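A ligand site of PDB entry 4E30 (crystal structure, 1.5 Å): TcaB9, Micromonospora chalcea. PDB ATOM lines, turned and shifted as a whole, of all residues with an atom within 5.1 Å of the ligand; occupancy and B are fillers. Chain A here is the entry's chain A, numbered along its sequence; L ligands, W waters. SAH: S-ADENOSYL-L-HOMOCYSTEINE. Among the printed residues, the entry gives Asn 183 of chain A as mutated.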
ATOM      1  N   ARG A  70     -21.584  10.520 -12.590  1.00  0.00           N
ATOM      2  CA  ARG A  70     -21.674   9.374 -13.510  1.00  0.00           C
ATOM      3  C   ARG A  70     -21.239   9.725 -14.946  1.00  0.00           C
ATOM      4  O   ARG A  70     -20.646   8.927 -15.667  1.00  0.00           O
ATOM      5  CB  ARG A  70     -23.053   8.705 -13.436  1.00  0.00           C
ATOM      6  CG  ARG A  70     -24.189   9.632 -13.939  1.00  0.00           C
ATOM      7  CD  ARG A  70     -25.526   8.904 -13.770  1.00  0.00           C
ATOM      8  NE  ARG A  70     -26.640   9.715 -14.249  1.00  0.00           N
ATOM      9  CZ  ARG A  70     -27.908   9.297 -14.166  1.00  0.00           C
ATOM     10  NH1 ARG A  70     -28.191   8.106 -13.668  1.00  0.00           N
ATOM     11  NH2 ARG A  70     -28.907  10.080 -14.596  1.00  0.00           N
ATOM     12  N   PHE A  74     -19.013   7.428 -17.522  1.00  0.00           N
ATOM     13  CA  PHE A  74     -19.722   6.593 -18.483  1.00  0.00           C
ATOM     14  C   PHE A  74     -20.355   7.520 -19.528  1.00  0.00           C
ATOM     15  O   PHE A  74     -21.182   8.375 -19.187  1.00  0.00           O
ATOM     16  CB  PHE A  74     -20.767   5.784 -17.699  1.00  0.00           C
ATOM     17  CG  PHE A  74     -20.204   5.051 -16.515  1.00  0.00           C
ATOM     18  CD1 PHE A  74     -19.293   4.033 -16.741  1.00  0.00           C
ATOM     19  CD2 PHE A  74     -20.638   5.335 -15.237  1.00  0.00           C
ATOM     20  CE1 PHE A  74     -18.741   3.338 -15.689  1.00  0.00           C
ATOM     21  CE2 PHE A  74     -20.102   4.628 -14.127  1.00  0.00           C
ATOM     22  CZ  PHE A  74     -19.174   3.617 -14.394  1.00  0.00           C
ATOM     23  N   TYR A  78     -16.173   5.730 -23.146  1.00  0.00           N
ATOM     24  CA  TYR A  78     -15.738   4.764 -22.138  1.00  0.00           C
ATOM     25  C   TYR A  78     -15.102   3.526 -22.807  1.00  0.00           C
ATOM     26  O   TYR A  78     -15.711   2.923 -23.698  1.00  0.00           O
ATOM     27  CB  TYR A  78     -16.981   4.364 -21.348  1.00  0.00           C
ATOM     28  CG  TYR A  78     -16.715   3.365 -20.232  1.00  0.00           C
ATOM     29  CD1 TYR A  78     -17.210   2.071 -20.366  1.00  0.00           C
ATOM     30  CD2 TYR A  78     -16.006   3.750 -19.110  1.00  0.00           C
ATOM     31  CE1 TYR A  78     -17.014   1.163 -19.316  1.00  0.00           C
ATOM     32  CE2 TYR A  78     -15.780   2.838 -18.057  1.00  0.00           C
ATOM     33  CZ  TYR A  78     -16.306   1.577 -18.215  1.00  0.00           C
ATOM     34  OH  TYR A  78     -16.133   0.648 -17.205  1.00  0.00           O
ATOM     35  N   TYR A  80     -13.860   0.403 -21.695  1.00  0.00           N
ATOM     36  CA  TYR A  80     -13.683  -0.952 -21.155  1.00  0.00           C
ATOM     37  C   TYR A  80     -14.512  -1.892 -22.016  1.00  0.00           C
ATOM     38  O   TYR A  80     -15.713  -1.691 -22.233  1.00  0.00           O
ATOM     39  CB  TYR A  80     -14.312  -1.075 -19.777  1.00  0.00           C
ATOM     40  CG  TYR A  80     -14.101  -2.448 -19.185  1.00  0.00           C
ATOM     41  CD1 TYR A  80     -12.814  -2.909 -18.929  1.00  0.00           C
ATOM     42  CD2 TYR A  80     -15.181  -3.281 -18.869  1.00  0.00           C
ATOM     43  CE1 TYR A  80     -12.580  -4.173 -18.392  1.00  0.00           C
ATOM     44  CE2 TYR A  80     -14.947  -4.545 -18.332  1.00  0.00           C
ATOM     45  CZ  TYR A  80     -13.654  -4.974 -18.103  1.00  0.00           C
ATOM     46  OH  TYR A  80     -13.378  -6.206 -17.530  1.00  0.00           O
ATOM     47  N   SER A  82     -15.718  -5.652 -22.201  1.00  0.00           N
ATOM     48  CA  SER A  82     -15.759  -6.854 -21.377  1.00  0.00           C
ATOM     49  C   SER A  82     -15.279  -8.067 -22.152  1.00  0.00           C
ATOM     50  O   SER A  82     -14.638  -8.951 -21.553  1.00  0.00           O
ATOM     51  CB  SER A  82     -17.203  -7.114 -20.952  1.00  0.00           C
ATOM     52  OG  SER A  82     -17.753  -5.988 -20.291  1.00  0.00           O
ATOM     53  N   PHE A  92     -19.780 -15.587 -18.526  1.00  0.00           N
ATOM     54  CA  PHE A  92     -21.094 -15.009 -18.711  1.00  0.00           C
ATOM     55  C   PHE A  92     -22.039 -15.887 -19.538  1.00  0.00           C
ATOM     56  O   PHE A  92     -23.240 -15.916 -19.303  1.00  0.00           O
ATOM     57  CB  PHE A  92     -21.034 -13.562 -19.275  1.00  0.00           C
ATOM     58  CG  PHE A  92     -20.522 -12.561 -18.268  1.00  0.00           C
ATOM     59  CD1 PHE A  92     -21.251 -12.329 -17.106  1.00  0.00           C
ATOM     60  CD2 PHE A  92     -19.303 -11.906 -18.472  1.00  0.00           C
ATOM     61  CE1 PHE A  92     -20.805 -11.420 -16.144  1.00  0.00           C
ATOM     62  CE2 PHE A  92     -18.835 -11.003 -17.502  1.00  0.00           C
ATOM     63  CZ  PHE A  92     -19.616 -10.737 -16.356  1.00  0.00           C
ATOM     64  N   GLU A 113     -30.561  -6.532 -18.375  1.00  0.00           N
ATOM     65  CA  GLU A 113     -29.226  -6.469 -17.805  1.00  0.00           C
ATOM     66  C   GLU A 113     -28.844  -4.988 -17.627  1.00  0.00           C
ATOM     67  O   GLU A 113     -28.989  -4.194 -18.545  1.00  0.00           O
ATOM     68  CB  GLU A 113     -28.182  -7.081 -18.739  1.00  0.00           C
ATOM     69  CG  GLU A 113     -26.838  -7.042 -18.033  1.00  0.00           C
ATOM     70  CD  GLU A 113     -25.699  -7.760 -18.740  1.00  0.00           C
ATOM     71  OE1 GLU A 113     -24.663  -8.020 -18.099  1.00  0.00           O
ATOM     72  OE2 GLU A 113     -25.847  -8.105 -19.934  1.00  0.00           O
ATOM     73  N   ILE A 114     -28.374  -4.645 -16.424  1.00  0.00           N
ATOM     74  CA  ILE A 114     -27.851  -3.298 -16.127  1.00  0.00           C
ATOM     75  C   ILE A 114     -26.351  -3.364 -16.378  1.00  0.00           C
ATOM     76  O   ILE A 114     -25.618  -4.131 -15.724  1.00  0.00           O
ATOM     77  CB  ILE A 114     -28.103  -3.015 -14.611  1.00  0.00           C
ATOM     78  CG1 ILE A 114     -29.603  -3.131 -14.327  1.00  0.00           C
ATOM     79  CG2 ILE A 114     -27.526  -1.632 -14.260  1.00  0.00           C
ATOM     80  CD1 ILE A 114     -30.054  -2.782 -12.902  1.00  0.00           C
ATOM     81  N   GLY A 115     -25.841  -2.555 -17.311  1.00  0.00           N
ATOM     82  CA  GLY A 115     -24.402  -2.584 -17.589  1.00  0.00           C
ATOM     83  C   GLY A 115     -23.987  -3.624 -18.605  1.00  0.00           C
ATOM     84  O   GLY A 115     -22.950  -4.275 -18.406  1.00  0.00           O
ATOM     85  N   CYS A 116     -24.734  -3.801 -19.695  1.00  0.00           N
ATOM     86  CA  CYS A 116     -24.489  -4.902 -20.636  1.00  0.00           C
ATOM     87  C   CYS A 116     -23.185  -4.794 -21.417  1.00  0.00           C
ATOM     88  O   CYS A 116     -22.688  -5.790 -21.964  1.00  0.00           O
ATOM     89  CB  CYS A 116     -25.709  -5.186 -21.537  1.00  0.00           C
ATOM     90  SG  CYS A 116     -25.986  -3.891 -22.729  1.00  0.00           S
ATOM     91  N   ASN A 117     -22.604  -3.593 -21.456  1.00  0.00           N
ATOM     92  CA  ASN A 117     -21.388  -3.307 -22.198  1.00  0.00           C
ATOM     93  C   ASN A 117     -21.514  -3.828 -23.618  1.00  0.00           C
ATOM     94  O   ASN A 117     -22.532  -3.580 -24.258  1.00  0.00           O
ATOM     95  CB  ASN A 117     -20.244  -3.928 -21.367  1.00  0.00           C
ATOM     96  CG  ASN A 117     -18.852  -3.398 -21.747  1.00  0.00           C
ATOM     97  OD1 ASN A 117     -18.156  -4.001 -22.548  1.00  0.00           O
ATOM     98  ND2 ASN A 117     -18.415  -2.303 -21.117  1.00  0.00           N
ATOM     99  N   ILE A 120     -21.448  -9.131 -23.792  1.00  0.00           N
ATOM    100  CA  ILE A 120     -20.825 -10.382 -23.290  1.00  0.00           C
ATOM    101  C   ILE A 120     -21.808 -11.402 -22.697  1.00  0.00           C
ATOM    102  O   ILE A 120     -21.645 -12.624 -22.865  1.00  0.00           O
ATOM    103  CB  ILE A 120     -19.679 -10.042 -22.288  1.00  0.00           C
ATOM    104  CG1 ILE A 120     -18.788 -11.274 -22.026  1.00  0.00           C
ATOM    105  CG2 ILE A 120     -20.215  -9.335 -21.008  1.00  0.00           C
ATOM    106  CD1 ILE A 120     -17.439 -10.909 -21.414  1.00  0.00           C
ATOM    107  N   PHE A 135     -29.230  -2.214 -20.576  1.00  0.00           N
ATOM    108  CA  PHE A 135     -29.036  -0.781 -20.324  1.00  0.00           C
ATOM    109  C   PHE A 135     -27.538  -0.555 -20.353  1.00  0.00           C
ATOM    110  O   PHE A 135     -26.769  -1.217 -19.636  1.00  0.00           O
ATOM    111  CB  PHE A 135     -29.493  -0.371 -18.929  1.00  0.00           C
ATOM    112  CG  PHE A 135     -30.973  -0.096 -18.825  1.00  0.00           C
ATOM    113  CD1 PHE A 135     -31.438   1.203 -18.911  1.00  0.00           C
ATOM    114  CD2 PHE A 135     -31.877  -1.139 -18.619  1.00  0.00           C
ATOM    115  CE1 PHE A 135     -32.805   1.470 -18.801  1.00  0.00           C
ATOM    116  CE2 PHE A 135     -33.264  -0.879 -18.521  1.00  0.00           C
ATOM    117  CZ  PHE A 135     -33.716   0.440 -18.615  1.00  0.00           C
ATOM    118  N   GLU A 136     -27.129   0.391 -21.196  1.00  0.00           N
ATOM    119  CA  GLU A 136     -25.692   0.629 -21.368  1.00  0.00           C
ATOM    120  C   GLU A 136     -25.547   2.113 -21.717  1.00  0.00           C
ATOM    121  O   GLU A 136     -25.670   2.449 -22.912  1.00  0.00           O
ATOM    122  CB  GLU A 136     -25.057  -0.312 -22.392  1.00  0.00           C
ATOM    123  CG  GLU A 136     -23.557  -0.175 -22.598  1.00  0.00           C
ATOM    124  CD  GLU A 136     -22.901   0.053 -21.245  1.00  0.00           C
ATOM    125  OE1 GLU A 136     -22.762  -0.955 -20.537  1.00  0.00           O
ATOM    126  OE2 GLU A 136     -22.634   1.200 -20.845  1.00  0.00           O
ATOM    127  N   PRO A 137     -25.238   2.951 -20.729  1.00  0.00           N
ATOM    128  CA  PRO A 137     -25.157   4.388 -20.996  1.00  0.00           C
ATOM    129  C   PRO A 137     -23.904   4.790 -21.738  1.00  0.00           C
ATOM    130  O   PRO A 137     -23.823   5.955 -22.118  1.00  0.00           O
ATOM    131  CB  PRO A 137     -25.158   5.007 -19.592  1.00  0.00           C
ATOM    132  CG  PRO A 137     -24.447   3.918 -18.743  1.00  0.00           C
ATOM    133  CD  PRO A 137     -25.151   2.700 -19.284  1.00  0.00           C
ATOM    134  N   SER A 138     -22.938   3.883 -21.888  1.00  0.00           N
ATOM    135  CA  SER A 138     -21.722   4.141 -22.662  1.00  0.00           C
ATOM    136  C   SER A 138     -21.963   3.714 -24.100  1.00  0.00           C
ATOM    137  O   SER A 138     -21.982   2.532 -24.416  1.00  0.00           O
ATOM    138  CB  SER A 138     -20.484   3.492 -22.046  1.00  0.00           C
ATOM    139  OG  SER A 138     -20.317   4.064 -20.754  1.00  0.00           O
ATOM    140  N   VAL A 141     -19.659   1.206 -26.454  1.00  0.00           N
ATOM    141  CA  VAL A 141     -19.723  -0.239 -26.203  1.00  0.00           C
ATOM    142  C   VAL A 141     -21.159  -0.697 -26.443  1.00  0.00           C
ATOM    143  O   VAL A 141     -21.384  -1.832 -26.885  1.00  0.00           O
ATOM    144  CB  VAL A 141     -19.188  -0.646 -24.797  1.00  0.00           C
ATOM    145  CG1 VAL A 141     -17.692  -0.462 -24.712  1.00  0.00           C
ATOM    146  CG2 VAL A 141     -19.966   0.105 -23.707  1.00  0.00           C
ATOM    147  N   ASP A 155     -28.939   4.289 -21.824  1.00  0.00           N
ATOM    148  CA  ASP A 155     -29.432   5.125 -20.733  1.00  0.00           C
ATOM    149  C   ASP A 155     -28.855   4.457 -19.484  1.00  0.00           C
ATOM    150  O   ASP A 155     -28.549   3.261 -19.469  1.00  0.00           O
ATOM    151  CB  ASP A 155     -30.943   4.947 -20.545  1.00  0.00           C
ATOM    152  CG  ASP A 155     -31.761   5.972 -21.306  1.00  0.00           C
ATOM    153  OD1 ASP A 155     -32.634   5.530 -22.087  1.00  0.00           O
ATOM    154  OD2 ASP A 155     -31.504   7.183 -21.128  1.00  0.00           O
ATOM    155  N   PHE A 156     -28.787   5.218 -18.400  1.00  0.00           N
ATOM    156  CA  PHE A 156     -28.556   4.637 -17.079  1.00  0.00           C
ATOM    157  C   PHE A 156     -29.842   4.007 -16.592  1.00  0.00           C
ATOM    158  O   PHE A 156     -30.927   4.567 -16.710  1.00  0.00           O
ATOM    159  CB  PHE A 156     -28.232   5.802 -16.137  1.00  0.00           C
ATOM    160  CG  PHE A 156     -26.910   6.482 -16.451  1.00  0.00           C
ATOM    161  CD1 PHE A 156     -25.715   5.895 -16.066  1.00  0.00           C
ATOM    162  CD2 PHE A 156     -26.848   7.691 -17.142  1.00  0.00           C
ATOM    163  CE1 PHE A 156     -24.468   6.482 -16.352  1.00  0.00           C
ATOM    164  CE2 PHE A 156     -25.616   8.287 -17.442  1.00  0.00           C
ATOM    165  CZ  PHE A 156     -24.427   7.694 -17.035  1.00  0.00           C
ATOM    166  N   PHE A 157     -29.732   2.800 -16.053  1.00  0.00           N
ATOM    167  CA  PHE A 157     -30.783   2.265 -15.196  1.00  0.00           C
ATOM    168  C   PHE A 157     -30.904   3.073 -13.909  1.00  0.00           C
ATOM    169  O   PHE A 157     -29.949   3.298 -13.160  1.00  0.00           O
ATOM    170  CB  PHE A 157     -30.524   0.771 -14.925  1.00  0.00           C
ATOM    171  CG  PHE A 157     -31.673   0.071 -14.258  1.00  0.00           C
ATOM    172  CD1 PHE A 157     -31.884   0.187 -12.889  1.00  0.00           C
ATOM    173  CD2 PHE A 157     -32.537  -0.700 -15.032  1.00  0.00           C
ATOM    174  CE1 PHE A 157     -32.942  -0.495 -12.267  1.00  0.00           C
ATOM    175  CE2 PHE A 157     -33.604  -1.371 -14.400  1.00  0.00           C
ATOM    176  CZ  PHE A 157     -33.808  -1.275 -13.031  1.00  0.00           C
ATOM    177  N   ALA A 178     -23.612  -7.211 -13.615  1.00  0.00           N
ATOM    178  CA  ALA A 178     -22.306  -7.694 -13.174  1.00  0.00           C
ATOM    179  C   ALA A 178     -21.273  -6.579 -13.160  1.00  0.00           C
ATOM    180  O   ALA A 178     -21.144  -5.900 -14.188  1.00  0.00           O
ATOM    181  CB  ALA A 178     -21.813  -8.819 -14.094  1.00  0.00           C
ATOM    182  N   ASN A 179     -20.521  -6.421 -12.057  1.00  0.00           N
ATOM    183  CA  ASN A 179     -19.461  -5.400 -12.036  1.00  0.00           C
ATOM    184  C   ASN A 179     -19.989  -4.013 -12.351  1.00  0.00           C
ATOM    185  O   ASN A 179     -19.216  -3.155 -12.797  1.00  0.00           O
ATOM    186  CB  ASN A 179     -18.354  -5.790 -13.039  1.00  0.00           C
ATOM    187  CG  ASN A 179     -17.828  -7.179 -12.694  1.00  0.00           C
ATOM    188  OD1 ASN A 179     -17.392  -7.330 -11.551  1.00  0.00           O
ATOM    189  ND2 ASN A 179     -17.931  -8.132 -13.624  1.00  0.00           N
ATOM    190  N   THR A 180     -21.261  -3.828 -12.019  1.00  0.00           N
ATOM    191  CA  THR A 180     -21.952  -2.567 -12.332  1.00  0.00           C
ATOM    192  C   THR A 180     -22.665  -1.982 -11.101  1.00  0.00           C
ATOM    193  O   THR A 180     -22.638  -0.747 -10.885  1.00  0.00           O
ATOM    194  CB  THR A 180     -22.987  -2.819 -13.456  1.00  0.00           C
ATOM    195  OG1 THR A 180     -22.264  -3.304 -14.592  1.00  0.00           O
ATOM    196  CG2 THR A 180     -23.727  -1.567 -13.888  1.00  0.00           C
ATOM    197  N   ASN A 183     -20.829   0.222  -8.876  1.00  0.00           N
ATOM    198  CA  ASN A 183     -20.382   1.481  -9.452  1.00  0.00           C
ATOM    199  C   ASN A 183     -21.360   2.612  -9.159  1.00  0.00           C
ATOM    200  O   ASN A 183     -21.051   3.768  -9.452  1.00  0.00           O
ATOM    201  CB  ASN A 183     -20.264   1.479 -10.974  1.00  0.00           C
ATOM    202  CG  ASN A 183     -19.504   0.350 -11.652  1.00  0.00           C
ATOM    203  OD1 ASN A 183     -19.248   0.504 -12.834  1.00  0.00           O
ATOM    204  ND2 ASN A 183     -19.083  -0.725 -10.987  1.00  0.00           N
ATOM    205  N   ILE A 184     -22.542   2.287  -8.647  1.00  0.00           N
ATOM    206  CA  ILE A 184     -23.689   3.193  -8.680  1.00  0.00           C
ATOM    207  C   ILE A 184     -24.019   3.741  -7.293  1.00  0.00           C
ATOM    208  O   ILE A 184     -24.630   3.057  -6.450  1.00  0.00           O
ATOM    209  CB  ILE A 184     -24.907   2.456  -9.282  1.00  0.00           C
ATOM    210  CG1 ILE A 184     -24.618   2.176 -10.765  1.00  0.00           C
ATOM    211  CG2 ILE A 184     -26.165   3.359  -9.205  1.00  0.00           C
ATOM    212  CD1 ILE A 184     -25.629   1.205 -11.432  1.00  0.00           C
ATOM    213  N   TYR A 186     -26.180   5.830  -6.473  1.00  0.00           N
ATOM    214  CA  TYR A 186     -27.645   5.974  -6.395  1.00  0.00           C
ATOM    215  C   TYR A 186     -28.381   4.644  -6.399  1.00  0.00           C
ATOM    216  O   TYR A 186     -29.377   4.433  -7.111  1.00  0.00           O
ATOM    217  CB  TYR A 186     -28.150   6.951  -7.473  1.00  0.00           C
ATOM    218  CG  TYR A 186     -27.605   6.647  -8.857  1.00  0.00           C
ATOM    219  CD1 TYR A 186     -26.357   7.082  -9.282  1.00  0.00           C
ATOM    220  CD2 TYR A 186     -28.409   5.939  -9.762  1.00  0.00           C
ATOM    221  CE1 TYR A 186     -25.928   6.806 -10.564  1.00  0.00           C
ATOM    222  CE2 TYR A 186     -27.996   5.634 -11.026  1.00  0.00           C
ATOM    223  CZ  TYR A 186     -26.725   6.057 -11.427  1.00  0.00           C
ATOM    224  OH  TYR A 186     -26.298   5.771 -12.699  1.00  0.00           O
ATOM    225  N   HIS A 256     -12.386 -11.704 -11.371  1.00  0.00           N
ATOM    226  CA  HIS A 256     -12.095 -10.351 -10.926  1.00  0.00           C
ATOM    227  C   HIS A 256     -11.483 -10.287  -9.520  1.00  0.00           C
ATOM    228  O   HIS A 256     -11.813  -9.333  -8.776  1.00  0.00           O
ATOM    229  CB  HIS A 256     -13.306  -9.440 -11.109  1.00  0.00           C
ATOM    230  CG  HIS A 256     -13.590  -9.144 -12.549  1.00  0.00           C
ATOM    231  ND1 HIS A 256     -12.669  -8.509 -13.354  1.00  0.00           N
ATOM    232  CD2 HIS A 256     -14.656  -9.406 -13.324  1.00  0.00           C
ATOM    233  CE1 HIS A 256     -13.166  -8.382 -14.572  1.00  0.00           C
ATOM    234  NE2 HIS A 256     -14.382  -8.922 -14.582  1.00  0.00           N
HETATM  235  N   SAH L   1     -21.158  -6.261 -17.077  1.00  0.00           N
HETATM  236  CA  SAH L   1     -19.919  -5.967 -17.837  1.00  0.00           C
HETATM  237  CB  SAH L   1     -19.581  -4.470 -17.759  1.00  0.00           C
HETATM  238  CG  SAH L   1     -19.012  -3.974 -16.424  1.00  0.00           C
HETATM  239  SD  SAH L   1     -18.357  -2.324 -16.510  1.00  0.00           S
HETATM  240  C   SAH L   1     -18.894  -6.866 -17.207  1.00  0.00           C
HETATM  241  O   SAH L   1     -19.127  -7.440 -16.129  1.00  0.00           O
HETATM  242  OXT SAH L   1     -17.775  -6.970 -17.733  1.00  0.00           O
HETATM  243  C5' SAH L   1     -19.758  -1.449 -15.881  1.00  0.00           C
HETATM  244  C4' SAH L   1     -20.743  -1.021 -16.990  1.00  0.00           C
HETATM  245  O4' SAH L   1     -21.883  -0.397 -16.345  1.00  0.00           O
HETATM  246  C3' SAH L   1     -20.169  -0.004 -17.995  1.00  0.00           C
HETATM  247  O3' SAH L   1     -20.311  -0.480 -19.347  1.00  0.00           O
HETATM  248  C2' SAH L   1     -21.041   1.216 -17.727  1.00  0.00           C
HETATM  249  O2' SAH L   1     -21.308   2.147 -18.789  1.00  0.00           O
HETATM  250  C1' SAH L   1     -22.357   0.614 -17.247  1.00  0.00           C
HETATM  251  N9  SAH L   1     -23.138   1.483 -16.328  1.00  0.00           N
HETATM  252  C8  SAH L   1     -22.758   2.404 -15.412  1.00  0.00           C
HETATM  253  N7  SAH L   1     -23.789   2.966 -14.757  1.00  0.00           N
HETATM  254  C5  SAH L   1     -24.912   2.325 -15.208  1.00  0.00           C
HETATM  255  C6  SAH L   1     -26.362   2.369 -14.937  1.00  0.00           C
HETATM  256  N6  SAH L   1     -26.841   3.229 -14.021  1.00  0.00           N
HETATM  257  N1  SAH L   1     -27.110   1.539 -15.706  1.00  0.00           N
HETATM  258  C2  SAH L   1     -26.638   0.692 -16.642  1.00  0.00           C
HETATM  259  N3  SAH L   1     -25.337   0.559 -16.962  1.00  0.00           N
HETATM  260  C4  SAH L   1     -24.481   1.347 -16.225  1.00  0.00           C
HETATM  261  O   HOH W   1     -15.776  -8.605 -16.942  1.00  0.00           O
HETATM  262  O   HOH W   2     -23.979  -6.294 -16.112  1.00  0.00           O
HETATM  263  O   HOH W   3     -15.234  -2.083 -15.923  1.00  0.00           O
HETATM  264  O   HOH W   4     -23.789   5.418 -13.212  1.00  0.00           O
HETATM  265  O   HOH W   5     -22.103  -8.623 -18.169  1.00  0.00           O
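Phe 74 touches the ligand.
CE2 of Tyr 80 touches OXT of the ligand (3.8 Å).
Phe 92 touches the ligand (CZ to O, 3.3 Å).
Ile 114 touches the ligand.
Phe 135 touches the ligand.
Pro 137 touches the ligand (CD to N3, 3.2 Å).
Phe 156 touches the ligand (CD1 to N6, 3.5 Å).
OD1 of Asn 183 touches C5' of the ligand (3.7 Å).
Ile 184 touches the ligand (CD1 to N6, 3.5 Å).
Hydrophobic or aromatic side chains that line the ligand: Phe 74, Tyr 78, Tyr 80, Phe 92, Ile 114, Phe 135, Pro 137, Phe 156, Phe 157, Ala 178, Ile 184 and Tyr 186.
Within 4 Å of the ligand: Phe 74, Tyr 78, Tyr 80, Ser 82, Phe 92, Ile 114, Gly 115, Asn 117, Phe 135, Glu 136, Pro 137, Ser 138, Phe 156, Phe 157, Ala 178, Asn 179, Thr 180, Asn 183, Ile 184 and Tyr 186.
The nearest printed residue that does not touch the ligand is Glu 113 (4.1 Å).
OE2 of Glu 136 is in hydrogen-bond range of O2' of the ligand (2.6 Å).
The side-chain hydroxyl of Ser 82 lies within hydrogen-bond range of an oxygen (OXT) of the ligand.
The side-chain amide nitrogen (ND2) of Asn 179 sits at hydrogen-bond distance from an oxygen (O) of the ligand (2.9 Å).
N of the ligand is in hydrogen-bond range of O of Ala 178.
N6 of the ligand lies within hydrogen-bond range of OH of Tyr 186, at 2.9 Å.
O2' of the ligand is in hydrogen-bond range of OG of Ser 138, at 2.9 Å.
A nitrogen (N1) of the ligand lies within hydrogen-bond range of the backbone NH (N) of Phe 157 (2.9 Å).
The backbone carbonyl oxygen of Phe 157 is in hydrogen-bond range of a nitrogen (N6) of the ligand, 3.2 Å away.
The backbone NH (N) of Gly 115 is in hydrogen-bond range of a nitrogen (N3) of the ligand, 3.2 Å away.
The backbone carbonyl oxygen (O) of Gly 115 sits at hydrogen-bond distance from a nitrogen (N) of the ligand, 3.0 Å away.
The side-chain amide nitrogen (ND2) of Asn 117 sits at hydrogen-bond distance from an oxygen (O3') of the ligand, 3.2 Å away.
The side-chain hydroxyl (OG1) of Thr 180 lies close to an oxygen (O4') of the ligand, 3.4 Å away.
A sulfur (SD) of the ligand sits close to the side-chain hydroxyl (OH) of Tyr 78.
The side-chain carboxylate (OE2) of Glu 136 lies within hydrogen-bond range of the backbone NH (N) of Ser 138, at 2.9 Å.
OE1 of Glu 136 sits at hydrogen-bond distance from N of Asn 117 (2.8 Å).
The backbone NH of Ser 82 lies within hydrogen-bond range of the side-chain amide oxygen of Asn 117 (3.0 Å).
The side-chain amide nitrogen (ND2) of Asn 183 is in hydrogen-bond range of the backbone carbonyl oxygen (O) of Asn 179, at 3.0 Å.
The backbone carbonyl oxygen (O) of Ala 178 is in hydrogen-bond range of the side-chain hydroxyl (OG1) of Thr 180, 2.9 Å away.
OH of Tyr 186 sits at hydrogen-bond distance from NH1 of Arg 70 (3.2 Å).
The side-chain amide nitrogen (ND2) of Asn 117 sits at hydrogen-bond distance from the backbone carbonyl oxygen (O) of Tyr 80, 3.0 Å away.
The backbone NH of Phe 135 is in hydrogen-bond range of the backbone carbonyl oxygen of Glu 113 (2.8 Å).
Water W1 lies within hydrogen-bond range of OXT of the ligand, NE2 of His 256 and OH of Tyr 80.
Water W5 bridges the side-chain carboxylate of Glu 113 (2.6 Å) and a nitrogen (N) of the ligand (2.8 Å).
Water W4 bridges OH of Tyr 186 (2.6 Å) and N7 of the ligand (2.9 Å).
Water W3 lies within hydrogen-bond range of OH of Tyr 78 (3.1 Å) and SD of the ligand (3.2 Å).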
